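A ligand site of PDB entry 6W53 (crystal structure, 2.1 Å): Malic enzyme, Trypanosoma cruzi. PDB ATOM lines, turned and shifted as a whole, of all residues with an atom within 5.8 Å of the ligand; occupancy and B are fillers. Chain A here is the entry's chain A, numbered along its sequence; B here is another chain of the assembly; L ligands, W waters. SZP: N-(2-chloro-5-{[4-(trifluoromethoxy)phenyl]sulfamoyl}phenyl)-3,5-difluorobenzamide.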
ATOM      1  N   LEU A   6      -8.245  13.429 -15.695  1.00  0.00           N
ATOM      2  CA  LEU A   6      -7.889  12.077 -16.131  1.00  0.00           C
ATOM      3  C   LEU A   6      -8.583  11.803 -17.455  1.00  0.00           C
ATOM      4  O   LEU A   6      -7.963  11.147 -18.272  1.00  0.00           O
ATOM      5  CB  LEU A   6      -8.353  11.087 -15.048  1.00  0.00           C
ATOM      6  CG  LEU A   6      -7.518  11.050 -13.778  1.00  0.00           C
ATOM      7  CD1 LEU A   6      -8.137  10.044 -12.807  1.00  0.00           C
ATOM      8  CD2 LEU A   6      -6.078  10.668 -14.089  1.00  0.00           C
ATOM      9  N   THR A   7      -9.804  12.305 -17.653  1.00  0.00           N
ATOM     10  CA  THR A   7     -10.658  11.992 -18.840  1.00  0.00           C
ATOM     11  C   THR A   7     -10.356  12.931 -20.002  1.00  0.00           C
ATOM     12  O   THR A   7     -10.879  12.753 -21.089  1.00  0.00           O
ATOM     13  CB  THR A   7     -12.137  12.041 -18.414  1.00  0.00           C
ATOM     14  OG1 THR A   7     -12.336  13.357 -17.898  1.00  0.00           O
ATOM     15  CG2 THR A   7     -12.430  10.988 -17.368  1.00  0.00           C
ATOM     16  N   ASP A   8      -9.556  13.945 -19.755  1.00  0.00           N
ATOM     17  CA  ASP A   8      -9.112  14.881 -20.810  1.00  0.00           C
ATOM     18  C   ASP A   8      -7.735  14.404 -21.283  1.00  0.00           C
ATOM     19  O   ASP A   8      -6.801  14.536 -20.511  1.00  0.00           O
ATOM     20  CB  ASP A   8      -9.064  16.307 -20.267  1.00  0.00           C
ATOM     21  CG  ASP A   8      -8.720  17.297 -21.364  1.00  0.00           C
ATOM     22  OD1 ASP A   8      -8.061  16.900 -22.300  1.00  0.00           O
ATOM     23  OD2 ASP A   8      -9.168  18.431 -21.265  1.00  0.00           O
ATOM     24  N   ASN A  12      -4.240  14.979 -19.227  1.00  0.00           N
ATOM     25  CA  ASN A  12      -3.952  13.768 -18.440  1.00  0.00           C
ATOM     26  C   ASN A  12      -2.451  13.462 -18.506  1.00  0.00           C
ATOM     27  O   ASN A  12      -1.854  13.499 -19.574  1.00  0.00           O
ATOM     28  CB  ASN A  12      -4.832  12.578 -18.874  1.00  0.00           C
ATOM     29  CG  ASN A  12      -4.553  11.384 -17.996  1.00  0.00           C
ATOM     30  OD1 ASN A  12      -4.239  11.582 -16.828  1.00  0.00           O
ATOM     31  ND2 ASN A  12      -4.643  10.174 -18.547  1.00  0.00           N
ATOM     32  N   ARG A  13      -1.887  13.106 -17.372  1.00  0.00           N
ATOM     33  CA  ARG A  13      -0.478  12.676 -17.220  1.00  0.00           C
ATOM     34  C   ARG A  13      -0.367  11.262 -16.661  1.00  0.00           C
ATOM     35  O   ARG A  13       0.790  10.757 -16.531  1.00  0.00           O
ATOM     36  CB  ARG A  13       0.179  13.630 -16.210  1.00  0.00           C
ATOM     37  CG  ARG A  13       0.083  15.080 -16.660  1.00  0.00           C
ATOM     38  CD  ARG A  13       1.171  15.870 -15.957  1.00  0.00           C
ATOM     39  NE  ARG A  13       0.880  17.275 -16.056  1.00  0.00           N
ATOM     40  CZ  ARG A  13       1.508  18.237 -15.395  1.00  0.00           C
ATOM     41  NH1 ARG A  13       2.479  17.941 -14.553  1.00  0.00           N
ATOM     42  NH2 ARG A  13       1.145  19.486 -15.576  1.00  0.00           N
ATOM     43  N   GLY A  14      -1.479  10.668 -16.263  1.00  0.00           N
ATOM     44  CA  GLY A  14      -1.453   9.362 -15.578  1.00  0.00           C
ATOM     45  C   GLY A  14      -0.462   9.352 -14.441  1.00  0.00           C
ATOM     46  O   GLY A  14      -0.497  10.242 -13.600  1.00  0.00           O
ATOM     47  N   THR A  15       0.409   8.344 -14.396  1.00  0.00           N
ATOM     48  CA  THR A  15       1.305   8.104 -13.251  1.00  0.00           C
ATOM     49  C   THR A  15       2.320   9.229 -13.115  1.00  0.00           C
ATOM     50  O   THR A  15       3.042   9.186 -12.096  1.00  0.00           O
ATOM     51  CB  THR A  15       2.015   6.756 -13.387  1.00  0.00           C
ATOM     52  OG1 THR A  15       2.773   6.784 -14.594  1.00  0.00           O
ATOM     53  CG2 THR A  15       1.028   5.611 -13.367  1.00  0.00           C
ATOM     54  N   ALA A  16       2.396  10.175 -14.062  1.00  0.00           N
ATOM     55  CA  ALA A  16       3.365  11.282 -13.972  1.00  0.00           C
ATOM     56  C   ALA A  16       2.827  12.383 -13.055  1.00  0.00           C
ATOM     57  O   ALA A  16       3.581  13.274 -12.724  1.00  0.00           O
ATOM     58  CB  ALA A  16       3.731  11.847 -15.343  1.00  0.00           C
ATOM     59  N   ARG A  30      -7.098   7.360  -7.720  1.00  0.00           N
ATOM     60  CA  ARG A  30      -7.658   7.059  -9.072  1.00  0.00           C
ATOM     61  C   ARG A  30      -6.571   6.390  -9.920  1.00  0.00           C
ATOM     62  O   ARG A  30      -6.806   6.089 -11.076  1.00  0.00           O
ATOM     63  CB  ARG A  30      -8.225   8.344  -9.704  1.00  0.00           C
ATOM     64  CG  ARG A  30      -9.429   8.935  -8.958  1.00  0.00           C
ATOM     65  CD  ARG A  30     -10.661   8.018  -8.914  1.00  0.00           C
ATOM     66  NE  ARG A  30     -10.746   7.340 -10.216  1.00  0.00           N
ATOM     67  CZ  ARG A  30     -11.107   7.925 -11.358  1.00  0.00           C
ATOM     68  NH1 ARG A  30     -11.504   9.195 -11.369  1.00  0.00           N
ATOM     69  NH2 ARG A  30     -11.076   7.253 -12.507  1.00  0.00           N
ATOM     70  N   LEU A  31      -5.387   6.246  -9.349  1.00  0.00           N
ATOM     71  CA  LEU A  31      -4.191   5.743 -10.078  1.00  0.00           C
ATOM     72  C   LEU A  31      -3.482   4.785  -9.153  1.00  0.00           C
ATOM     73  O   LEU A  31      -3.494   5.000  -7.926  1.00  0.00           O
ATOM     74  CB  LEU A  31      -3.225   6.878 -10.416  1.00  0.00           C
ATOM     75  CG  LEU A  31      -3.743   7.902 -11.427  1.00  0.00           C
ATOM     76  CD1 LEU A  31      -2.950   9.177 -11.276  1.00  0.00           C
ATOM     77  CD2 LEU A  31      -3.647   7.340 -12.849  1.00  0.00           C
ATOM     78  N   PRO A  32      -2.729   3.824  -9.711  1.00  0.00           N
ATOM     79  CA  PRO A  32      -1.816   3.027  -8.909  1.00  0.00           C
ATOM     80  C   PRO A  32      -0.764   3.951  -8.290  1.00  0.00           C
ATOM     81  O   PRO A  32      -0.565   5.065  -8.786  1.00  0.00           O
ATOM     82  CB  PRO A  32      -1.229   2.015  -9.907  1.00  0.00           C
ATOM     83  CG  PRO A  32      -1.388   2.672 -11.257  1.00  0.00           C
ATOM     84  CD  PRO A  32      -2.618   3.545 -11.156  1.00  0.00           C
ATOM     85  N   GLU A  36       5.875   8.062 -12.046  1.00  0.00           N
ATOM     86  CA  GLU A  36       6.867   7.956 -13.152  1.00  0.00           C
ATOM     87  C   GLU A  36       7.118   9.325 -13.762  1.00  0.00           C
ATOM     88  O   GLU A  36       6.233  10.189 -13.697  1.00  0.00           O
ATOM     89  CB  GLU A  36       6.355   7.026 -14.241  1.00  0.00           C
ATOM     90  CG  GLU A  36       6.480   5.563 -13.868  1.00  0.00           C
ATOM     91  CD  GLU A  36       5.618   4.668 -14.745  1.00  0.00           C
ATOM     92  OE1 GLU A  36       4.432   5.019 -14.941  1.00  0.00           O
ATOM     93  OE2 GLU A  36       6.143   3.650 -15.261  1.00  0.00           O
ATOM     94  N   GLN A  41       7.429   6.494 -18.526  1.00  0.00           N
ATOM     95  CA  GLN A  41       6.109   6.113 -19.068  1.00  0.00           C
ATOM     96  C   GLN A  41       6.333   5.609 -20.487  1.00  0.00           C
ATOM     97  O   GLN A  41       5.687   4.604 -20.904  1.00  0.00           O
ATOM     98  CB  GLN A  41       5.157   7.298 -19.047  1.00  0.00           C
ATOM     99  CG  GLN A  41       4.804   7.749 -17.643  1.00  0.00           C
ATOM    100  CD  GLN A  41       3.816   8.873 -17.737  1.00  0.00           C
ATOM    101  OE1 GLN A  41       4.154   9.924 -18.267  1.00  0.00           O
ATOM    102  NE2 GLN A  41       2.593   8.643 -17.255  1.00  0.00           N
ATOM    103  N   ARG A  44       7.731   2.176 -20.630  1.00  0.00           N
ATOM    104  CA  ARG A  44       6.648   1.226 -20.226  1.00  0.00           C
ATOM    105  C   ARG A  44       5.738   0.986 -21.432  1.00  0.00           C
ATOM    106  O   ARG A  44       5.553  -0.165 -21.828  1.00  0.00           O
ATOM    107  CB  ARG A  44       5.871   1.750 -19.025  1.00  0.00           C
ATOM    108  CG  ARG A  44       4.797   0.800 -18.531  1.00  0.00           C
ATOM    109  CD  ARG A  44       4.307   1.093 -17.157  1.00  0.00           C
ATOM    110  NE  ARG A  44       3.997   2.499 -16.920  1.00  0.00           N
ATOM    111  CZ  ARG A  44       2.933   3.153 -17.388  1.00  0.00           C
ATOM    112  NH1 ARG A  44       2.090   2.578 -18.216  1.00  0.00           N
ATOM    113  NH2 ARG A  44       2.727   4.419 -17.019  1.00  0.00           N
ATOM    114  N   VAL A  45       5.315   2.052 -22.079  1.00  0.00           N
ATOM    115  CA  VAL A  45       4.434   1.967 -23.265  1.00  0.00           C
ATOM    116  C   VAL A  45       5.168   1.167 -24.330  1.00  0.00           C
ATOM    117  O   VAL A  45       4.549   0.254 -24.899  1.00  0.00           O
ATOM    118  CB  VAL A  45       3.975   3.348 -23.772  1.00  0.00           C
ATOM    119  CG1 VAL A  45       3.243   3.209 -25.103  1.00  0.00           C
ATOM    120  CG2 VAL A  45       3.103   4.068 -22.746  1.00  0.00           C
ATOM    121  N   GLN A  48       4.870  -2.362 -23.659  1.00  0.00           N
ATOM    122  CA  GLN A  48       3.466  -2.765 -23.902  1.00  0.00           C
ATOM    123  C   GLN A  48       3.282  -3.017 -25.417  1.00  0.00           C
ATOM    124  O   GLN A  48       2.705  -4.033 -25.772  1.00  0.00           O
ATOM    125  CB  GLN A  48       2.507  -1.710 -23.358  1.00  0.00           C
ATOM    126  CG  GLN A  48       2.347  -1.693 -21.840  1.00  0.00           C
ATOM    127  CD  GLN A  48       1.747  -0.410 -21.326  1.00  0.00           C
ATOM    128  OE1 GLN A  48       1.778  -0.121 -20.109  1.00  0.00           O
ATOM    129  NE2 GLN A  48       1.224   0.377 -22.254  1.00  0.00           N
ATOM    130  N   HIS A  61      -2.996  -0.863 -29.881  1.00  0.00           N
ATOM    131  CA  HIS A  61      -2.526  -0.409 -28.554  1.00  0.00           C
ATOM    132  C   HIS A  61      -2.214   1.090 -28.612  1.00  0.00           C
ATOM    133  O   HIS A  61      -2.666   1.859 -27.741  1.00  0.00           O
ATOM    134  CB  HIS A  61      -1.317  -1.215 -28.083  1.00  0.00           C
ATOM    135  CG  HIS A  61      -0.907  -0.775 -26.729  1.00  0.00           C
ATOM    136  ND1 HIS A  61      -1.769  -0.859 -25.664  1.00  0.00           N
ATOM    137  CD2 HIS A  61       0.223  -0.186 -26.277  1.00  0.00           C
ATOM    138  CE1 HIS A  61      -1.169  -0.365 -24.589  1.00  0.00           C
ATOM    139  NE2 HIS A  61       0.062   0.035 -24.929  1.00  0.00           N
ATOM    140  N   SER A  64      -5.211   3.468 -28.400  1.00  0.00           N
ATOM    141  CA  SER A  64      -5.731   3.536 -27.018  1.00  0.00           C
ATOM    142  C   SER A  64      -4.818   4.414 -26.124  1.00  0.00           C
ATOM    143  O   SER A  64      -5.337   5.235 -25.331  1.00  0.00           O
ATOM    144  CB  SER A  64      -5.978   2.116 -26.540  1.00  0.00           C
ATOM    145  OG  SER A  64      -6.216   2.118 -25.152  1.00  0.00           O
ATOM    146  N   VAL A  65      -3.492   4.378 -26.290  1.00  0.00           N
ATOM    147  CA  VAL A  65      -2.553   5.353 -25.637  1.00  0.00           C
ATOM    148  C   VAL A  65      -2.941   6.792 -26.043  1.00  0.00           C
ATOM    149  O   VAL A  65      -3.213   7.620 -25.116  1.00  0.00           O
ATOM    150  CB  VAL A  65      -1.069   5.045 -25.937  1.00  0.00           C
ATOM    151  CG1 VAL A  65      -0.147   6.035 -25.239  1.00  0.00           C
ATOM    152  CG2 VAL A  65      -0.671   3.611 -25.553  1.00  0.00           C
ATOM    153  N   THR A  68      -6.047   8.171 -24.233  1.00  0.00           N
ATOM    154  CA  THR A  68      -5.950   8.302 -22.763  1.00  0.00           C
ATOM    155  C   THR A  68      -5.031   9.457 -22.384  1.00  0.00           C
ATOM    156  O   THR A  68      -5.348  10.190 -21.438  1.00  0.00           O
ATOM    157  CB  THR A  68      -5.442   6.977 -22.159  1.00  0.00           C
ATOM    158  OG1 THR A  68      -6.303   5.940 -22.618  1.00  0.00           O
ATOM    159  CG2 THR A  68      -5.408   7.028 -20.649  1.00  0.00           C
ATOM    160  N   ASN A  69      -3.858   9.514 -23.026  1.00  0.00           N
ATOM    161  CA  ASN A  69      -2.739  10.422 -22.671  1.00  0.00           C
ATOM    162  C   ASN A  69      -2.031  10.761 -23.981  1.00  0.00           C
ATOM    163  O   ASN A  69      -1.161   9.996 -24.440  1.00  0.00           O
ATOM    164  CB  ASN A  69      -1.852   9.770 -21.626  1.00  0.00           C
ATOM    165  CG  ASN A  69      -0.723  10.651 -21.138  1.00  0.00           C
ATOM    166  OD1 ASN A  69      -0.391  11.645 -21.778  1.00  0.00           O
ATOM    167  ND2 ASN A  69      -0.137  10.271 -20.000  1.00  0.00           N
ATOM    168  N   LEU A  72       1.861  11.422 -23.909  1.00  0.00           N
ATOM    169  CA  LEU A  72       2.610  10.146 -23.836  1.00  0.00           C
ATOM    170  C   LEU A  72       2.628   9.439 -25.193  1.00  0.00           C
ATOM    171  O   LEU A  72       3.657   8.755 -25.531  1.00  0.00           O
ATOM    172  CB  LEU A  72       1.959   9.255 -22.775  1.00  0.00           C
ATOM    173  CG  LEU A  72       2.585   7.883 -22.567  1.00  0.00           C
ATOM    174  CD1 LEU A  72       4.061   7.976 -22.240  1.00  0.00           C
ATOM    175  CD2 LEU A  72       1.866   7.140 -21.459  1.00  0.00           C
ATOM    176  N   TYR A 545       5.036  17.343 -20.617  1.00  0.00           N
ATOM    177  CA  TYR A 545       3.971  17.838 -19.704  1.00  0.00           C
ATOM    178  C   TYR A 545       4.225  19.328 -19.387  1.00  0.00           C
ATOM    179  O   TYR A 545       5.160  19.605 -18.640  1.00  0.00           O
ATOM    180  CB  TYR A 545       3.895  16.929 -18.487  1.00  0.00           C
ATOM    181  CG  TYR A 545       3.521  15.484 -18.749  1.00  0.00           C
ATOM    182  CD1 TYR A 545       2.337  15.145 -19.400  1.00  0.00           C
ATOM    183  CD2 TYR A 545       4.351  14.451 -18.329  1.00  0.00           C
ATOM    184  CE1 TYR A 545       1.983  13.826 -19.621  1.00  0.00           C
ATOM    185  CE2 TYR A 545       4.000  13.122 -18.523  1.00  0.00           C
ATOM    186  CZ  TYR A 545       2.806  12.807 -19.164  1.00  0.00           C
ATOM    187  OH  TYR A 545       2.524  11.498 -19.429  1.00  0.00           O
ATOM    188  N   HIS B 102      -2.695  -3.013 -18.763  1.00  0.00           N
ATOM    189  CA  HIS B 102      -2.969  -1.717 -19.440  1.00  0.00           C
ATOM    190  C   HIS B 102      -4.395  -1.694 -19.990  1.00  0.00           C
ATOM    191  O   HIS B 102      -4.879  -0.612 -20.184  1.00  0.00           O
ATOM    192  CB  HIS B 102      -1.931  -1.414 -20.558  1.00  0.00           C
ATOM    193  CG  HIS B 102      -1.914  -2.398 -21.672  1.00  0.00           C
ATOM    194  ND1 HIS B 102      -1.066  -3.474 -21.671  1.00  0.00           N
ATOM    195  CD2 HIS B 102      -2.667  -2.502 -22.792  1.00  0.00           C
ATOM    196  CE1 HIS B 102      -1.286  -4.228 -22.738  1.00  0.00           C
ATOM    197  NE2 HIS B 102      -2.253  -3.631 -23.460  1.00  0.00           N
ATOM    198  N   LEU B 103      -5.064  -2.827 -20.207  1.00  0.00           N
ATOM    199  CA  LEU B 103      -6.437  -2.847 -20.772  1.00  0.00           C
ATOM    200  C   LEU B 103      -7.444  -2.291 -19.763  1.00  0.00           C
ATOM    201  O   LEU B 103      -8.580  -2.017 -20.136  1.00  0.00           O
ATOM    202  CB  LEU B 103      -6.776  -4.290 -21.159  1.00  0.00           C
ATOM    203  CG  LEU B 103      -5.990  -4.860 -22.339  1.00  0.00           C
ATOM    204  CD1 LEU B 103      -6.363  -6.310 -22.565  1.00  0.00           C
ATOM    205  CD2 LEU B 103      -6.193  -4.036 -23.601  1.00  0.00           C
ATOM    206  N   PHE B 104      -7.049  -2.130 -18.498  1.00  0.00           N
ATOM    207  CA  PHE B 104      -7.913  -1.601 -17.405  1.00  0.00           C
ATOM    208  C   PHE B 104      -7.588  -0.149 -17.035  1.00  0.00           C
ATOM    209  O   PHE B 104      -8.329   0.431 -16.191  1.00  0.00           O
ATOM    210  CB  PHE B 104      -7.798  -2.522 -16.188  1.00  0.00           C
ATOM    211  CG  PHE B 104      -8.148  -3.942 -16.520  1.00  0.00           C
ATOM    212  CD1 PHE B 104      -9.465  -4.297 -16.743  1.00  0.00           C
ATOM    213  CD2 PHE B 104      -7.173  -4.903 -16.715  1.00  0.00           C
ATOM    214  CE1 PHE B 104      -9.785  -5.590 -17.087  1.00  0.00           C
ATOM    215  CE2 PHE B 104      -7.495  -6.218 -17.029  1.00  0.00           C
ATOM    216  CZ  PHE B 104      -8.810  -6.554 -17.215  1.00  0.00           C
ATOM    217  N   PHE B 105      -6.597   0.479 -17.669  1.00  0.00           N
ATOM    218  CA  PHE B 105      -6.144   1.813 -17.216  1.00  0.00           C
ATOM    219  C   PHE B 105      -7.258   2.876 -17.321  1.00  0.00           C
ATOM    220  O   PHE B 105      -7.267   3.783 -16.492  1.00  0.00           O
ATOM    221  CB  PHE B 105      -4.904   2.308 -17.954  1.00  0.00           C
ATOM    222  CG  PHE B 105      -3.621   1.591 -17.614  1.00  0.00           C
ATOM    223  CD1 PHE B 105      -3.492   0.813 -16.484  1.00  0.00           C
ATOM    224  CD2 PHE B 105      -2.510   1.742 -18.448  1.00  0.00           C
ATOM    225  CE1 PHE B 105      -2.286   0.171 -16.190  1.00  0.00           C
ATOM    226  CE2 PHE B 105      -1.293   1.149 -18.138  1.00  0.00           C
ATOM    227  CZ  PHE B 105      -1.200   0.331 -17.033  1.00  0.00           C
ATOM    228  N   ARG B 106      -8.137   2.803 -18.314  1.00  0.00           N
ATOM    229  CA  ARG B 106      -9.094   3.892 -18.628  1.00  0.00           C
ATOM    230  C   ARG B 106     -10.390   3.713 -17.831  1.00  0.00           C
ATOM    231  O   ARG B 106     -11.320   4.520 -18.037  1.00  0.00           O
ATOM    232  CB  ARG B 106      -9.498   3.835 -20.113  1.00  0.00           C
ATOM    233  CG  ARG B 106      -8.343   3.900 -21.112  1.00  0.00           C
ATOM    234  CD  ARG B 106      -8.686   3.559 -22.569  1.00  0.00           C
ATOM    235  NE  ARG B 106      -9.202   4.599 -23.476  1.00  0.00           N
ATOM    236  CZ  ARG B 106      -9.722   5.809 -23.158  1.00  0.00           C
ATOM    237  NH1 ARG B 106     -10.142   6.591 -24.140  1.00  0.00           N
ATOM    238  NH2 ARG B 106      -9.836   6.272 -21.920  1.00  0.00           N
ATOM    239  N   GLU B 107     -10.480   2.659 -17.019  1.00  0.00           N
ATOM    240  CA  GLU B 107     -11.729   2.283 -16.298  1.00  0.00           C
ATOM    241  C   GLU B 107     -11.700   2.958 -14.929  1.00  0.00           C
ATOM    242  O   GLU B 107     -10.694   2.885 -14.224  1.00  0.00           O
ATOM    243  CB  GLU B 107     -11.905   0.770 -16.195  1.00  0.00           C
ATOM    244  CG  GLU B 107     -11.825   0.070 -17.542  1.00  0.00           C
ATOM    245  CD  GLU B 107     -12.606   0.711 -18.683  1.00  0.00           C
ATOM    246  OE1 GLU B 107     -13.741   1.150 -18.453  1.00  0.00           O
ATOM    247  OE2 GLU B 107     -12.068   0.763 -19.813  1.00  0.00           O
ATOM    248  N   ARG B 108     -12.785   3.622 -14.604  1.00  0.00           N
ATOM    249  CA  ARG B 108     -12.896   4.396 -13.370  1.00  0.00           C
ATOM    250  C   ARG B 108     -12.831   3.374 -12.265  1.00  0.00           C
ATOM    251  O   ARG B 108     -13.626   2.461 -12.288  1.00  0.00           O
ATOM    252  CB  ARG B 108     -14.212   5.173 -13.412  1.00  0.00           C
ATOM    253  CG  ARG B 108     -14.388   6.194 -12.301  1.00  0.00           C
ATOM    254  CD  ARG B 108     -15.656   6.928 -12.645  1.00  0.00           C
ATOM    255  NE  ARG B 108     -16.040   7.903 -11.635  1.00  0.00           N
ATOM    256  CZ  ARG B 108     -17.290   8.279 -11.381  1.00  0.00           C
ATOM    257  NH1 ARG B 108     -18.310   7.724 -12.033  1.00  0.00           N
ATOM    258  NH2 ARG B 108     -17.544   9.189 -10.450  1.00  0.00           N
ATOM    259  N   GLY B 109     -11.874   3.521 -11.363  1.00  0.00           N
ATOM    260  CA  GLY B 109     -11.828   2.707 -10.159  1.00  0.00           C
ATOM    261  C   GLY B 109     -11.061   3.388  -9.050  1.00  0.00           C
ATOM    262  O   GLY B 109     -10.669   4.544  -9.195  1.00  0.00           O
ATOM    263  N   TYR B 111      -8.118   2.879  -6.022  1.00  0.00           N
ATOM    264  CA  TYR B 111      -6.912   2.156  -5.553  1.00  0.00           C
ATOM    265  C   TYR B 111      -6.661   2.553  -4.093  1.00  0.00           C
ATOM    266  O   TYR B 111      -6.423   3.738  -3.798  1.00  0.00           O
ATOM    267  CB  TYR B 111      -5.723   2.551  -6.425  1.00  0.00           C
ATOM    268  CG  TYR B 111      -5.861   2.218  -7.877  1.00  0.00           C
ATOM    269  CD1 TYR B 111      -6.716   2.935  -8.701  1.00  0.00           C
ATOM    270  CD2 TYR B 111      -5.092   1.221  -8.449  1.00  0.00           C
ATOM    271  CE1 TYR B 111      -6.809   2.644 -10.061  1.00  0.00           C
ATOM    272  CE2 TYR B 111      -5.194   0.901  -9.789  1.00  0.00           C
ATOM    273  CZ  TYR B 111      -6.047   1.636 -10.598  1.00  0.00           C
ATOM    274  OH  TYR B 111      -6.096   1.369 -11.926  1.00  0.00           O
ATOM    275  N   LEU B 196       3.036  -1.224 -11.227  1.00  0.00           N
ATOM    276  CA  LEU B 196       2.656   0.129 -10.719  1.00  0.00           C
ATOM    277  C   LEU B 196       2.104   0.047  -9.295  1.00  0.00           C
ATOM    278  O   LEU B 196       1.768   1.131  -8.714  1.00  0.00           O
ATOM    279  CB  LEU B 196       1.629   0.725 -11.705  1.00  0.00           C
ATOM    280  CG  LEU B 196       2.144   0.766 -13.131  1.00  0.00           C
ATOM    281  CD1 LEU B 196       1.073   1.285 -14.039  1.00  0.00           C
ATOM    282  CD2 LEU B 196       3.399   1.636 -13.194  1.00  0.00           C
HETATM  283  N1  SZP L   1       0.043   5.231 -19.030  1.00  0.00           N
HETATM  284  C4  SZP L   1     -10.037   7.432 -16.801  1.00  0.00           C
HETATM  285  C5  SZP L   1      -9.456   6.706 -15.777  1.00  0.00           C
HETATM  286  C6  SZP L   1      -8.072   6.598 -15.628  1.00  0.00           C
HETATM  287  C7  SZP L   1      -3.859   5.452 -16.058  1.00  0.00           C
HETATM  288  C8  SZP L   1      -2.846   6.016 -16.892  1.00  0.00           C
HETATM  289  C10 SZP L   1      -1.197   4.490 -16.086  1.00  0.00           C
HETATM  290  C13 SZP L   1      -2.042   5.118 -20.240  1.00  0.00           C
HETATM  291  C15 SZP L   1      -0.122   3.781 -20.804  1.00  0.00           C
HETATM  292  C17 SZP L   1      -2.132   3.554 -22.096  1.00  0.00           C
HETATM  293 CL   SZP L   1      -4.643   3.648 -14.174  1.00  0.00          CL
HETATM  294  C19 SZP L   1      -3.463   4.391 -15.232  1.00  0.00           C
HETATM  295  N   SZP L   1      -5.166   5.887 -15.927  1.00  0.00           N
HETATM  296  C   SZP L   1      -5.725   7.027 -16.445  1.00  0.00           C
HETATM  297  C1  SZP L   1      -7.219   7.205 -16.523  1.00  0.00           C
HETATM  298  F1  SZP L   1     -10.256   6.103 -14.873  1.00  0.00           F
HETATM  299  C3  SZP L   1      -9.193   8.060 -17.695  1.00  0.00           C
HETATM  300  F   SZP L   1      -9.756   8.767 -18.675  1.00  0.00           F
HETATM  301  C2  SZP L   1      -7.785   7.949 -17.574  1.00  0.00           C
HETATM  302  O   SZP L   1      -5.102   7.932 -16.969  1.00  0.00           O
HETATM  303  C11 SZP L   1      -2.184   3.914 -15.253  1.00  0.00           C
HETATM  304  C9  SZP L   1      -1.518   5.534 -16.966  1.00  0.00           C
HETATM  305  S   SZP L   1      -0.361   6.247 -17.941  1.00  0.00           S
HETATM  306  O2  SZP L   1      -0.927   7.479 -18.486  1.00  0.00           O
HETATM  307  O3  SZP L   1       0.643   6.554 -16.951  1.00  0.00           O
HETATM  308  C12 SZP L   1      -0.732   4.757 -20.005  1.00  0.00           C
HETATM  309  C16 SZP L   1      -0.825   3.174 -21.821  1.00  0.00           C
HETATM  310  C14 SZP L   1      -2.751   4.525 -21.296  1.00  0.00           C
HETATM  311  O1  SZP L   1      -2.790   2.969 -23.156  1.00  0.00           O
HETATM  312  C18 SZP L   1      -3.841   2.074 -22.866  1.00  0.00           C
HETATM  313  F2  SZP L   1      -3.319   1.151 -22.114  1.00  0.00           F
HETATM  314  F3  SZP L   1      -4.210   1.508 -23.952  1.00  0.00           F
HETATM  315  F4  SZP L   1      -4.869   2.675 -22.329  1.00  0.00           F
HETATM  316  O   HOH W   1     -12.624   8.632 -14.407  1.00  0.00           O
HETATM  317  O   HOH W   2      -7.837  10.616 -20.754  1.00  0.00           O
HETATM  318  O   HOH W   3      -9.064   5.084 -12.093  1.00  0.00           O
HETATM  319  O   HOH W   4      -8.057   3.149 -13.786  1.00  0.00           O
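The side-chain hydroxyl of Thr 68 is in hydrogen-bond range of the backbone carbonyl oxygen of Ser 64 (3.0 Å).
The backbone carbonyl oxygen (O) of Leu 6 lies close to the side-chain amide nitrogen (ND2) of Asn 12 (3.5 Å).
NE2 of Gln 41 is in hydrogen-bond range of O of Arg 13, at 2.9 Å.
NE of Arg 106 of chain B lies close to OG1 of Thr 68 (3.3 Å).
The side-chain amide nitrogen (ND2) of Asn 69 sits at hydrogen-bond distance from the side-chain hydroxyl (OH) of Tyr 545, at 3.0 Å.
OH of Tyr 545 lies within hydrogen-bond range of OE1 of Gln 41, 2.5 Å away.
The guanidinium group of Arg 44 lies within salt-bridge range of the side-chain carboxylate of Glu 36 (2.8 Å).
NH2 of Arg 44 sits at hydrogen-bond distance from OG1 of Thr 15, at 3.4 Å.
The guanidinium group (NH2) of Arg 44 is in hydrogen-bond range of an oxygen (O3) of the ligand, at 3.0 Å.
An oxygen (O3) of the ligand is in hydrogen-bond range of the side-chain amide nitrogen (NE2) of Gln 41.
The backbone NH (N) of Thr 15 lies within hydrogen-bond range of an oxygen (O3) of the ligand, at 3.1 Å.
N of the ligand is in hydrogen-bond range of O of Phe 105 of chain B (3.0 Å).
The side-chain amide nitrogen (ND2) of Asn 12 lies within hydrogen-bond range of an oxygen (O) of the ligand, 2.8 Å away.
The side-chain hydroxyl of Thr 15 sits at hydrogen-bond distance from an oxygen (O3) of the ligand, 3.2 Å away.
The side-chain amide nitrogen of Asn 69 is in hydrogen-bond range of an oxygen (O2) of the ligand (3.3 Å).
O of Leu 6 sits close to F of the ligand, at 3.0 Å.
The guanidinium group (NH2) of Arg 30 sits close to a fluorine (F1) of the ligand.
A fluorine (F3) of the ligand sits close to the side-chain hydroxyl of Ser 64 (2.4 Å).
The backbone carbonyl oxygen of His 102 of chain B lies close to a fluorine (F2) of the ligand (3.0 Å).
The backbone carbonyl oxygen (O) of Glu 107 of chain B lies close to a fluorine (F1) of the ligand, 3.3 Å away.
Residues that only touch the ligand: Val 65, Thr 7, Arg 106 of chain B, Arg 108 of chain B, Gln 48, Gly 14, Tyr 111 of chain B, Thr 68, Leu 72, His 61, Pro 32, Leu 31 and Val 45.
24 residues have an atom within 4 Å of the ligand: Leu 6, Thr 7, Asn 12, Gly 14, Thr 15, Arg 30, Leu 31, Pro 32, Gln 41, Arg 44, Val 45, Gln 48, His 61, Ser 64, Val 65, Thr 68, Asn 69, Leu 72, His 102 of chain B, Phe 105 of chain B, Arg 106 of chain B, Glu 107 of chain B, Arg 108 of chain B and Tyr 111 of chain B.
The nearest printed residue that does not touch the ligand is Arg 13 (4.2 Å).
Water W3 lies within hydrogen-bond range of the backbone carbonyl oxygen of Arg 30 (2.7 Å), the backbone NH of Gly 109 of chain B (3.3 Å) and the backbone carbonyl oxygen of Glu 107 of chain B (3.5 Å).
Water W2 bridges O of Leu 6 (2.5 Å) and O of Thr 68 (2.6 Å).
Water W4 lies within hydrogen-bond range of O of Glu 107 of chain B, O of Phe 105 of chain B and OH of Tyr 111 of chain B.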
